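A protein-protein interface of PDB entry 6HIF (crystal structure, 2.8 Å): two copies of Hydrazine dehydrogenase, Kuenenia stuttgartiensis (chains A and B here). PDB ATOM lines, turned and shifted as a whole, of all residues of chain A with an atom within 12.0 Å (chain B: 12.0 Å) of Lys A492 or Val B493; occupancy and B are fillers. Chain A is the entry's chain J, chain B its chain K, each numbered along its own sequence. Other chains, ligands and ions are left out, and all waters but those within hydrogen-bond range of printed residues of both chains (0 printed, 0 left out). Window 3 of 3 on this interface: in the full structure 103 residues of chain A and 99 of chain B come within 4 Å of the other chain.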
ATOM      1  N   VAL A 384      42.378  -3.248 -19.023  1.00  0.00           N
ATOM      2  CA  VAL A 384      41.018  -3.596 -18.636  1.00  0.00           C
ATOM      3  C   VAL A 384      41.024  -4.753 -17.638  1.00  0.00           C
ATOM      4  O   VAL A 384      39.960  -5.206 -17.219  1.00  0.00           O
ATOM      5  CB  VAL A 384      40.124  -3.888 -19.858  1.00  0.00           C
ATOM      6  CG1 VAL A 384      39.804  -2.624 -20.639  1.00  0.00           C
ATOM      7  CG2 VAL A 384      40.715  -4.947 -20.774  1.00  0.00           C
ATOM      8  N   ALA A 483      35.252  -9.155 -18.156  1.00  0.00           N
ATOM      9  CA  ALA A 483      35.964  -7.964 -17.722  1.00  0.00           C
ATOM     10  C   ALA A 483      35.949  -6.900 -18.819  1.00  0.00           C
ATOM     11  O   ALA A 483      35.896  -5.709 -18.524  1.00  0.00           O
ATOM     12  CB  ALA A 483      37.371  -8.328 -17.325  1.00  0.00           C
ATOM     13  N   ARG A 484      35.996  -7.348 -20.079  1.00  0.00           N
ATOM     14  CA  ARG A 484      36.032  -6.460 -21.228  1.00  0.00           C
ATOM     15  C   ARG A 484      34.646  -5.878 -21.478  1.00  0.00           C
ATOM     16  O   ARG A 484      34.523  -4.735 -21.916  1.00  0.00           O
ATOM     17  CB  ARG A 484      36.556  -7.200 -22.464  1.00  0.00           C
ATOM     18  CG  ARG A 484      38.066  -7.384 -22.476  1.00  0.00           C
ATOM     19  CD  ARG A 484      38.568  -7.968 -23.781  1.00  0.00           C
ATOM     20  NE  ARG A 484      39.989  -8.284 -23.731  1.00  0.00           N
ATOM     21  CZ  ARG A 484      40.974  -7.424 -23.969  1.00  0.00           C
ATOM     22  NH1 ARG A 484      40.707  -6.167 -24.277  1.00  0.00           N
ATOM     23  NH2 ARG A 484      42.230  -7.818 -23.894  1.00  0.00           N
ATOM     24  N   ARG A 485      33.612  -6.682 -21.200  1.00  0.00           N
ATOM     25  CA  ARG A 485      32.232  -6.274 -21.408  1.00  0.00           C
ATOM     26  C   ARG A 485      31.838  -5.215 -20.380  1.00  0.00           C
ATOM     27  O   ARG A 485      31.082  -4.301 -20.701  1.00  0.00           O
ATOM     28  CB  ARG A 485      31.287  -7.479 -21.361  1.00  0.00           C
ATOM     29  CG  ARG A 485      31.318  -8.339 -22.614  1.00  0.00           C
ATOM     30  CD  ARG A 485      29.924  -8.764 -23.027  1.00  0.00           C
ATOM     31  NE  ARG A 485      29.435  -9.999 -22.437  1.00  0.00           N
ATOM     32  CZ  ARG A 485      28.180 -10.426 -22.532  1.00  0.00           C
ATOM     33  NH1 ARG A 485      27.263  -9.685 -23.126  1.00  0.00           N
ATOM     34  NH2 ARG A 485      27.842 -11.597 -22.026  1.00  0.00           N
ATOM     35  N   LEU A 486      32.361  -5.353 -19.153  1.00  0.00           N
ATOM     36  CA  LEU A 486      32.083  -4.421 -18.072  1.00  0.00           C
ATOM     37  C   LEU A 486      32.786  -3.090 -18.333  1.00  0.00           C
ATOM     38  O   LEU A 486      32.204  -2.031 -18.111  1.00  0.00           O
ATOM     39  CB  LEU A 486      32.538  -5.023 -16.737  1.00  0.00           C
ATOM     40  CG  LEU A 486      31.629  -6.097 -16.144  1.00  0.00           C
ATOM     41  CD1 LEU A 486      32.346  -6.834 -15.023  1.00  0.00           C
ATOM     42  CD2 LEU A 486      30.325  -5.502 -15.635  1.00  0.00           C
ATOM     43  N   ALA A 487      34.038  -3.163 -18.801  1.00  0.00           N
ATOM     44  CA  ALA A 487      34.843  -1.986 -19.082  1.00  0.00           C
ATOM     45  C   ALA A 487      34.202  -1.161 -20.197  1.00  0.00           C
ATOM     46  O   ALA A 487      34.216   0.067 -20.145  1.00  0.00           O
ATOM     47  CB  ALA A 487      36.248  -2.401 -19.440  1.00  0.00           C
ATOM     48  N   ALA A 488      33.638  -1.853 -21.195  1.00  0.00           N
ATOM     49  CA  ALA A 488      32.995  -1.216 -22.335  1.00  0.00           C
ATOM     50  C   ALA A 488      31.722  -0.497 -21.889  1.00  0.00           C
ATOM     51  O   ALA A 488      31.458   0.620 -22.330  1.00  0.00           O
ATOM     52  CB  ALA A 488      32.712  -2.235 -23.413  1.00  0.00           C
ATOM     53  N   LEU A 489      30.952  -1.149 -21.006  1.00  0.00           N
ATOM     54  CA  LEU A 489      29.702  -0.606 -20.499  1.00  0.00           C
ATOM     55  C   LEU A 489      29.979   0.629 -19.646  1.00  0.00           C
ATOM     56  O   LEU A 489      29.251   1.613 -19.723  1.00  0.00           O
ATOM     57  CB  LEU A 489      28.974  -1.681 -19.683  1.00  0.00           C
ATOM     58  CG  LEU A 489      28.091  -2.643 -20.477  1.00  0.00           C
ATOM     59  CD1 LEU A 489      27.812  -3.898 -19.669  1.00  0.00           C
ATOM     60  CD2 LEU A 489      26.784  -1.981 -20.880  1.00  0.00           C
ATOM     61  N   GLU A 490      31.043   0.567 -18.841  1.00  0.00           N
ATOM     62  CA  GLU A 490      31.360   1.629 -17.899  1.00  0.00           C
ATOM     63  C   GLU A 490      31.869   2.860 -18.645  1.00  0.00           C
ATOM     64  O   GLU A 490      31.652   3.986 -18.201  1.00  0.00           O
ATOM     65  CB  GLU A 490      32.370   1.138 -16.861  1.00  0.00           C
ATOM     66  CG  GLU A 490      31.756   0.231 -15.813  1.00  0.00           C
ATOM     67  CD  GLU A 490      32.744  -0.531 -14.948  1.00  0.00           C
ATOM     68  OE1 GLU A 490      33.906  -0.683 -15.365  1.00  0.00           O
ATOM     69  OE2 GLU A 490      32.341  -0.971 -13.854  1.00  0.00           O
ATOM     70  N   LYS A 491      32.553   2.634 -19.770  1.00  0.00           N
ATOM     71  CA  LYS A 491      33.042   3.728 -20.590  1.00  0.00           C
ATOM     72  C   LYS A 491      31.851   4.497 -21.158  1.00  0.00           C
ATOM     73  O   LYS A 491      31.796   5.720 -21.046  1.00  0.00           O
ATOM     74  CB  LYS A 491      33.996   3.219 -21.677  1.00  0.00           C
ATOM     75  CG  LYS A 491      34.356   4.239 -22.752  1.00  0.00           C
ATOM     76  CD  LYS A 491      35.522   3.844 -23.627  1.00  0.00           C
ATOM     77  CE  LYS A 491      36.854   4.264 -23.045  1.00  0.00           C
ATOM     78  NZ  LYS A 491      37.956   4.036 -24.006  1.00  0.00           N
ATOM     79  N   LYS A 492      30.891   3.763 -21.734  1.00  0.00           N
ATOM     80  CA  LYS A 492      29.778   4.355 -22.461  1.00  0.00           C
ATOM     81  C   LYS A 492      28.826   5.069 -21.502  1.00  0.00           C
ATOM     82  O   LYS A 492      28.234   6.082 -21.860  1.00  0.00           O
ATOM     83  CB  LYS A 492      29.058   3.300 -23.308  1.00  0.00           C
ATOM     84  CG  LYS A 492      28.058   3.851 -24.319  1.00  0.00           C
ATOM     85  CD  LYS A 492      27.894   2.970 -25.540  1.00  0.00           C
ATOM     86  CE  LYS A 492      26.632   3.247 -26.330  1.00  0.00           C
ATOM     87  NZ  LYS A 492      26.714   4.536 -27.059  1.00  0.00           N
ATOM     88  N   VAL A 493      28.685   4.537 -20.287  1.00  0.00           N
ATOM     89  CA  VAL A 493      27.771   5.096 -19.302  1.00  0.00           C
ATOM     90  C   VAL A 493      28.493   6.196 -18.521  1.00  0.00           C
ATOM     91  O   VAL A 493      27.855   7.022 -17.871  1.00  0.00           O
ATOM     92  CB  VAL A 493      27.191   3.990 -18.396  1.00  0.00           C
ATOM     93  CG1 VAL A 493      26.479   4.540 -17.170  1.00  0.00           C
ATOM     94  CG2 VAL A 493      26.263   3.075 -19.176  1.00  0.00           C
ATOM     95  N   GLY A 494      29.829   6.201 -18.604  1.00  0.00           N
ATOM     96  CA  GLY A 494      30.642   7.238 -17.991  1.00  0.00           C
ATOM     97  C   GLY A 494      30.978   6.946 -16.530  1.00  0.00           C
ATOM     98  O   GLY A 494      31.172   7.872 -15.746  1.00  0.00           O
ATOM     99  N   ILE A 495      31.042   5.654 -16.176  1.00  0.00           N
ATOM    100  CA  ILE A 495      31.543   5.232 -14.877  1.00  0.00           C
ATOM    101  C   ILE A 495      33.032   4.939 -15.025  1.00  0.00           C
ATOM    102  O   ILE A 495      33.442   4.214 -15.929  1.00  0.00           O
ATOM    103  CB  ILE A 495      30.780   4.007 -14.326  1.00  0.00           C
ATOM    104  CG1 ILE A 495      29.277   4.272 -14.208  1.00  0.00           C
ATOM    105  CG2 ILE A 495      31.370   3.547 -12.996  1.00  0.00           C
ATOM    106  CD1 ILE A 495      28.451   3.042 -13.896  1.00  0.00           C
ATOM    107  N   SER A 496      33.832   5.530 -14.137  1.00  0.00           N
ATOM    108  CA  SER A 496      35.205   5.098 -13.974  1.00  0.00           C
ATOM    109  C   SER A 496      35.275   4.201 -12.746  1.00  0.00           C
ATOM    110  O   SER A 496      35.120   4.664 -11.617  1.00  0.00           O
ATOM    111  CB  SER A 496      36.127   6.267 -13.868  1.00  0.00           C
ATOM    112  OG  SER A 496      37.489   5.868 -13.832  1.00  0.00           O
ATOM    113  N   TRP A 497      35.489   2.906 -13.001  1.00  0.00           N
ATOM    114  CA  TRP A 497      35.421   1.888 -11.970  1.00  0.00           C
ATOM    115  C   TRP A 497      36.554   2.067 -10.967  1.00  0.00           C
ATOM    116  O   TRP A 497      37.722   2.057 -11.341  1.00  0.00           O
ATOM    117  CB  TRP A 497      35.431   0.487 -12.593  1.00  0.00           C
ATOM    118  CG  TRP A 497      35.672  -0.601 -11.592  1.00  0.00           C
ATOM    119  CD1 TRP A 497      34.917  -0.891 -10.491  1.00  0.00           C
ATOM    120  CD2 TRP A 497      36.748  -1.555 -11.603  1.00  0.00           C
ATOM    121  NE1 TRP A 497      35.447  -1.958  -9.815  1.00  0.00           N
ATOM    122  CE2 TRP A 497      36.571  -2.386 -10.473  1.00  0.00           C
ATOM    123  CE3 TRP A 497      37.841  -1.784 -12.448  1.00  0.00           C
ATOM    124  CZ2 TRP A 497      37.446  -3.429 -10.176  1.00  0.00           C
ATOM    125  CZ3 TRP A 497      38.708  -2.813 -12.152  1.00  0.00           C
ATOM    126  CH2 TRP A 497      38.511  -3.622 -11.031  1.00  0.00           C
ATOM    127  N   ARG B 484      23.377 -12.828 -18.523  1.00  0.00           N
ATOM    128  CA  ARG B 484      22.058 -12.273 -18.780  1.00  0.00           C
ATOM    129  C   ARG B 484      22.022 -10.811 -18.341  1.00  0.00           C
ATOM    130  O   ARG B 484      21.358  -9.992 -18.973  1.00  0.00           O
ATOM    131  CB  ARG B 484      20.976 -13.100 -18.076  1.00  0.00           C
ATOM    132  CG  ARG B 484      20.645 -14.414 -18.770  1.00  0.00           C
ATOM    133  CD  ARG B 484      19.456 -15.125 -18.147  1.00  0.00           C
ATOM    134  NE  ARG B 484      19.233 -16.446 -18.716  1.00  0.00           N
ATOM    135  CZ  ARG B 484      18.554 -16.690 -19.831  1.00  0.00           C
ATOM    136  NH1 ARG B 484      17.998 -15.702 -20.507  1.00  0.00           N
ATOM    137  NH2 ARG B 484      18.437 -17.928 -20.276  1.00  0.00           N
ATOM    138  N   ARG B 485      22.744 -10.502 -17.256  1.00  0.00           N
ATOM    139  CA  ARG B 485      22.775  -9.161 -16.700  1.00  0.00           C
ATOM    140  C   ARG B 485      23.543  -8.227 -17.635  1.00  0.00           C
ATOM    141  O   ARG B 485      23.192  -7.055 -17.766  1.00  0.00           O
ATOM    142  CB  ARG B 485      23.387  -9.168 -15.296  1.00  0.00           C
ATOM    143  CG  ARG B 485      22.461  -9.708 -14.214  1.00  0.00           C
ATOM    144  CD  ARG B 485      22.511  -8.853 -12.962  1.00  0.00           C
ATOM    145  NE  ARG B 485      23.510  -9.219 -11.973  1.00  0.00           N
ATOM    146  CZ  ARG B 485      23.839  -8.472 -10.922  1.00  0.00           C
ATOM    147  NH1 ARG B 485      23.318  -7.269 -10.758  1.00  0.00           N
ATOM    148  NH2 ARG B 485      24.696  -8.928 -10.030  1.00  0.00           N
ATOM    149  N   LEU B 486      24.588  -8.762 -18.280  1.00  0.00           N
ATOM    150  CA  LEU B 486      25.403  -7.998 -19.208  1.00  0.00           C
ATOM    151  C   LEU B 486      24.620  -7.734 -20.492  1.00  0.00           C
ATOM    152  O   LEU B 486      24.672  -6.634 -21.031  1.00  0.00           O
ATOM    153  CB  LEU B 486      26.696  -8.765 -19.506  1.00  0.00           C
ATOM    154  CG  LEU B 486      27.762  -8.730 -18.411  1.00  0.00           C
ATOM    155  CD1 LEU B 486      28.844  -9.757 -18.694  1.00  0.00           C
ATOM    156  CD2 LEU B 486      28.372  -7.343 -18.284  1.00  0.00           C
ATOM    157  N   ALA B 487      23.900  -8.758 -20.968  1.00  0.00           N
ATOM    158  CA  ALA B 487      23.127  -8.667 -22.195  1.00  0.00           C
ATOM    159  C   ALA B 487      22.025  -7.623 -22.038  1.00  0.00           C
ATOM    160  O   ALA B 487      21.727  -6.896 -22.983  1.00  0.00           O
ATOM    161  CB  ALA B 487      22.561 -10.018 -22.557  1.00  0.00           C
ATOM    162  N   ALA B 488      21.439  -7.561 -20.835  1.00  0.00           N
ATOM    163  CA  ALA B 488      20.354  -6.638 -20.541  1.00  0.00           C
ATOM    164  C   ALA B 488      20.882  -5.205 -20.531  1.00  0.00           C
ATOM    165  O   ALA B 488      20.241  -4.304 -21.069  1.00  0.00           O
ATOM    166  CB  ALA B 488      19.696  -7.005 -19.233  1.00  0.00           C
ATOM    167  N   LEU B 489      22.060  -5.019 -19.923  1.00  0.00           N
ATOM    168  CA  LEU B 489      22.687  -3.712 -19.812  1.00  0.00           C
ATOM    169  C   LEU B 489      23.071  -3.208 -21.199  1.00  0.00           C
ATOM    170  O   LEU B 489      22.908  -2.030 -21.499  1.00  0.00           O
ATOM    171  CB  LEU B 489      23.917  -3.818 -18.909  1.00  0.00           C
ATOM    172  CG  LEU B 489      23.647  -3.693 -17.410  1.00  0.00           C
ATOM    173  CD1 LEU B 489      24.803  -4.265 -16.610  1.00  0.00           C
ATOM    174  CD2 LEU B 489      23.399  -2.245 -17.015  1.00  0.00           C
ATOM    175  N   GLU B 490      23.567  -4.117 -22.039  1.00  0.00           N
ATOM    176  CA  GLU B 490      24.074  -3.752 -23.351  1.00  0.00           C
ATOM    177  C   GLU B 490      22.923  -3.372 -24.280  1.00  0.00           C
ATOM    178  O   GLU B 490      23.085  -2.512 -25.141  1.00  0.00           O
ATOM    179  CB  GLU B 490      24.922  -4.884 -23.930  1.00  0.00           C
ATOM    180  CG  GLU B 490      26.299  -4.972 -23.299  1.00  0.00           C
ATOM    181  CD  GLU B 490      27.074  -6.241 -23.613  1.00  0.00           C
ATOM    182  OE1 GLU B 490      26.442  -7.236 -24.028  1.00  0.00           O
ATOM    183  OE2 GLU B 490      28.309  -6.230 -23.443  1.00  0.00           O
ATOM    184  N   LYS B 491      21.769  -4.024 -24.102  1.00  0.00           N
ATOM    185  CA  LYS B 491      20.587  -3.703 -24.883  1.00  0.00           C
ATOM    186  C   LYS B 491      20.149  -2.275 -24.564  1.00  0.00           C
ATOM    187  O   LYS B 491      19.935  -1.480 -25.478  1.00  0.00           O
ATOM    188  CB  LYS B 491      19.476  -4.734 -24.649  1.00  0.00           C
ATOM    189  CG  LYS B 491      18.115  -4.362 -25.230  1.00  0.00           C
ATOM    190  CD  LYS B 491      17.107  -5.492 -25.266  1.00  0.00           C
ATOM    191  CE  LYS B 491      17.186  -6.318 -26.534  1.00  0.00           C
ATOM    192  NZ  LYS B 491      16.060  -7.276 -26.629  1.00  0.00           N
ATOM    193  N   LYS B 492      20.056  -1.956 -23.265  1.00  0.00           N
ATOM    194  CA  LYS B 492      19.491  -0.696 -22.806  1.00  0.00           C
ATOM    195  C   LYS B 492      20.416   0.466 -23.164  1.00  0.00           C
ATOM    196  O   LYS B 492      19.945   1.559 -23.471  1.00  0.00           O
ATOM    197  CB  LYS B 492      19.191  -0.739 -21.305  1.00  0.00           C
ATOM    198  CG  LYS B 492      18.332   0.411 -20.792  1.00  0.00           C
ATOM    199  CD  LYS B 492      17.467   0.043 -19.607  1.00  0.00           C
ATOM    200  CE  LYS B 492      16.953   1.241 -18.836  1.00  0.00           C
ATOM    201  NZ  LYS B 492      15.897   1.968 -19.580  1.00  0.00           N
ATOM    202  N   VAL B 493      21.729   0.216 -23.131  1.00  0.00           N
ATOM    203  CA  VAL B 493      22.717   1.250 -23.398  1.00  0.00           C
ATOM    204  C   VAL B 493      22.987   1.322 -24.900  1.00  0.00           C
ATOM    205  O   VAL B 493      23.569   2.289 -25.382  1.00  0.00           O
ATOM    206  CB  VAL B 493      23.999   1.019 -22.576  1.00  0.00           C
ATOM    207  CG1 VAL B 493      25.157   1.885 -23.047  1.00  0.00           C
ATOM    208  CG2 VAL B 493      23.747   1.226 -21.090  1.00  0.00           C
ATOM    209  N   GLY B 494      22.556   0.293 -25.634  1.00  0.00           N
ATOM    210  CA  GLY B 494      22.648   0.291 -27.085  1.00  0.00           C
ATOM    211  C   GLY B 494      24.007  -0.191 -27.593  1.00  0.00           C
ATOM    212  O   GLY B 494      24.438   0.215 -28.670  1.00  0.00           O
ATOM    213  N   ILE B 495      24.671  -1.055 -26.812  1.00  0.00           N
ATOM    214  CA  ILE B 495      25.865  -1.751 -27.261  1.00  0.00           C
ATOM    215  C   ILE B 495      25.443  -3.104 -27.822  1.00  0.00           C
ATOM    216  O   ILE B 495      24.723  -3.857 -27.170  1.00  0.00           O
ATOM    217  CB  ILE B 495      26.897  -1.924 -26.127  1.00  0.00           C
ATOM    218  CG1 ILE B 495      27.305  -0.584 -25.511  1.00  0.00           C
ATOM    219  CG2 ILE B 495      28.105  -2.711 -26.618  1.00  0.00           C
ATOM    220  CD1 ILE B 495      28.124  -0.707 -24.247  1.00  0.00           C
ATOM    221  N   SER B 496      25.891  -3.388 -29.045  1.00  0.00           N
ATOM    222  CA  SER B 496      25.824  -4.732 -29.585  1.00  0.00           C
ATOM    223  C   SER B 496      27.188  -5.386 -29.388  1.00  0.00           C
ATOM    224  O   SER B 496      28.151  -5.014 -30.056  1.00  0.00           O
ATOM    225  CB  SER B 496      25.418  -4.702 -31.030  1.00  0.00           C
ATOM    226  OG  SER B 496      25.215  -6.016 -31.517  1.00  0.00           O
ATOM    227  N   TRP B 497      27.254  -6.337 -28.444  1.00  0.00           N
ATOM    228  CA  TRP B 497      28.507  -6.952 -28.032  1.00  0.00           C
ATOM    229  C   TRP B 497      29.111  -7.770 -29.170  1.00  0.00           C
ATOM    230  O   TRP B 497      28.477  -8.689 -29.686  1.00  0.00           O
ATOM    231  CB  TRP B 497      28.325  -7.799 -26.765  1.00  0.00           C
ATOM    232  CG  TRP B 497      29.497  -8.680 -26.447  1.00  0.00           C
ATOM    233  CD1 TRP B 497      30.780  -8.290 -26.187  1.00  0.00           C
ATOM    234  CD2 TRP B 497      29.491 -10.116 -26.342  1.00  0.00           C
ATOM    235  NE1 TRP B 497      31.572  -9.377 -25.928  1.00  0.00           N
ATOM    236  CE2 TRP B 497      30.809 -10.512 -26.017  1.00  0.00           C
ATOM    237  CE3 TRP B 497      28.509 -11.103 -26.493  1.00  0.00           C
ATOM    238  CZ2 TRP B 497      31.162 -11.851 -25.845  1.00  0.00           C
ATOM    239  CZ3 TRP B 497      28.859 -12.425 -26.322  1.00  0.00           C
ATOM    240  CH2 TRP B 497      30.168 -12.791 -26.004  1.00  0.00           C
ATOM    241  N   GLN B 498      30.348  -7.408 -29.535  1.00  0.00           N
ATOM    242  CA  GLN B 498      31.137  -8.147 -30.505  1.00  0.00           C
ATOM    243  C   GLN B 498      31.960  -9.194 -29.757  1.00  0.00           C
ATOM    244  O   GLN B 498      32.859  -8.837 -28.999  1.00  0.00           O
ATOM    245  CB  GLN B 498      32.043  -7.188 -31.280  1.00  0.00           C
ATOM    246  CG  GLN B 498      32.513  -7.738 -32.621  1.00  0.00           C
ATOM    247  CD  GLN B 498      31.462  -7.612 -33.699  1.00  0.00           C
ATOM    248  OE1 GLN B 498      30.963  -6.525 -33.984  1.00  0.00           O
ATOM    249  NE2 GLN B 498      31.122  -8.735 -34.315  1.00  0.00           N
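NH1 of Arg A485 is in salt-bridge range of OE1 of Glu B490 (2.7 Å).
The backbone carbonyl oxygen (O) of Glu B490 sits at hydrogen-bond distance from the backbone NH (N) of Ile B495 (2.7 Å).
Among the printed residues, pairs that only touch across the chains: Arg A485 with Trp B497 (3.3 Å), Lys A492 with Val B493 (3.3 Å), Lys A492 with Ile B495 (3.6 Å), Val A493 with Val B493 (3.7 Å), Leu A489 with Leu B486 (3.8 Å), Arg A485 with Leu B486 (3.8 Å), Leu A486 with Leu B486 (3.8 Å), Leu A489 with Ile B495 (3.8 Å), Leu A489 with Glu B490 (3.9 Å) and Leu A489 with Leu B489 (3.9 Å).
Ala A488 touches none of the printed residues of chain B. Of chain B, only Val B493 (3.3 Å) and Ile B495 (3.6 Å) come within 4 Å of Lys A492. No residue of chain B comes within 4 Å of Gly A494. Arg B484 touches none of the printed residues of chain A. Of the printed residues of chain A, Leu B486 touches Arg A485, Leu A486 and Leu A489. Of the printed residues of chain A, Glu B490 touches Arg A485 (2.7 Å) and Leu A489 (3.9 Å). No residue of chain A comes within 4 Å of Lys B492. Val B493 touches two residues of chain A. No residue of chain A comes within 4 Å of Gly B494. Of chain A, only Leu A489 (3.8 Å) and Lys A492 (3.6 Å) come within 4 Å of Ile B495. Ser B496 touches none of the printed residues of chain A. The nearest residue of chain B that does not touch Lys A492 is Gly B494 (4.4 Å).
Hydrophobic or aromatic side chains of chain A that line the printed part of chain B: Leu A486, Leu A489 and Val A493. Of the 15 printed residues of chain B, 6 touch a printed residue of chain A. Among the printed residues, Asp or Glu carboxylates within 4 Å of a Lys or Arg side-chain nitrogen of the other chain: Arg A485 with Glu B490.
Arg A485 touches Leu B486, but with the chains exchanged Leu A486 does not touch Arg B485 (7.6 Å). Arg A485 touches Trp B497, but with the chains exchanged Trp A497 does not touch Arg B485 (12.8 Å). Lys A492 touches Val B493, but with the chains exchanged Val A493 does not touch Lys B492 (7.5 Å). Lys A492 touches Ile B495, but with the chains exchanged Ile A495 does not touch Lys B492 (12.4 Å). Positions printed for both chains: 484, 485, 486, 487, 488, 489, 490, 491, 492, 493, 494, 495, 496 and 497.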
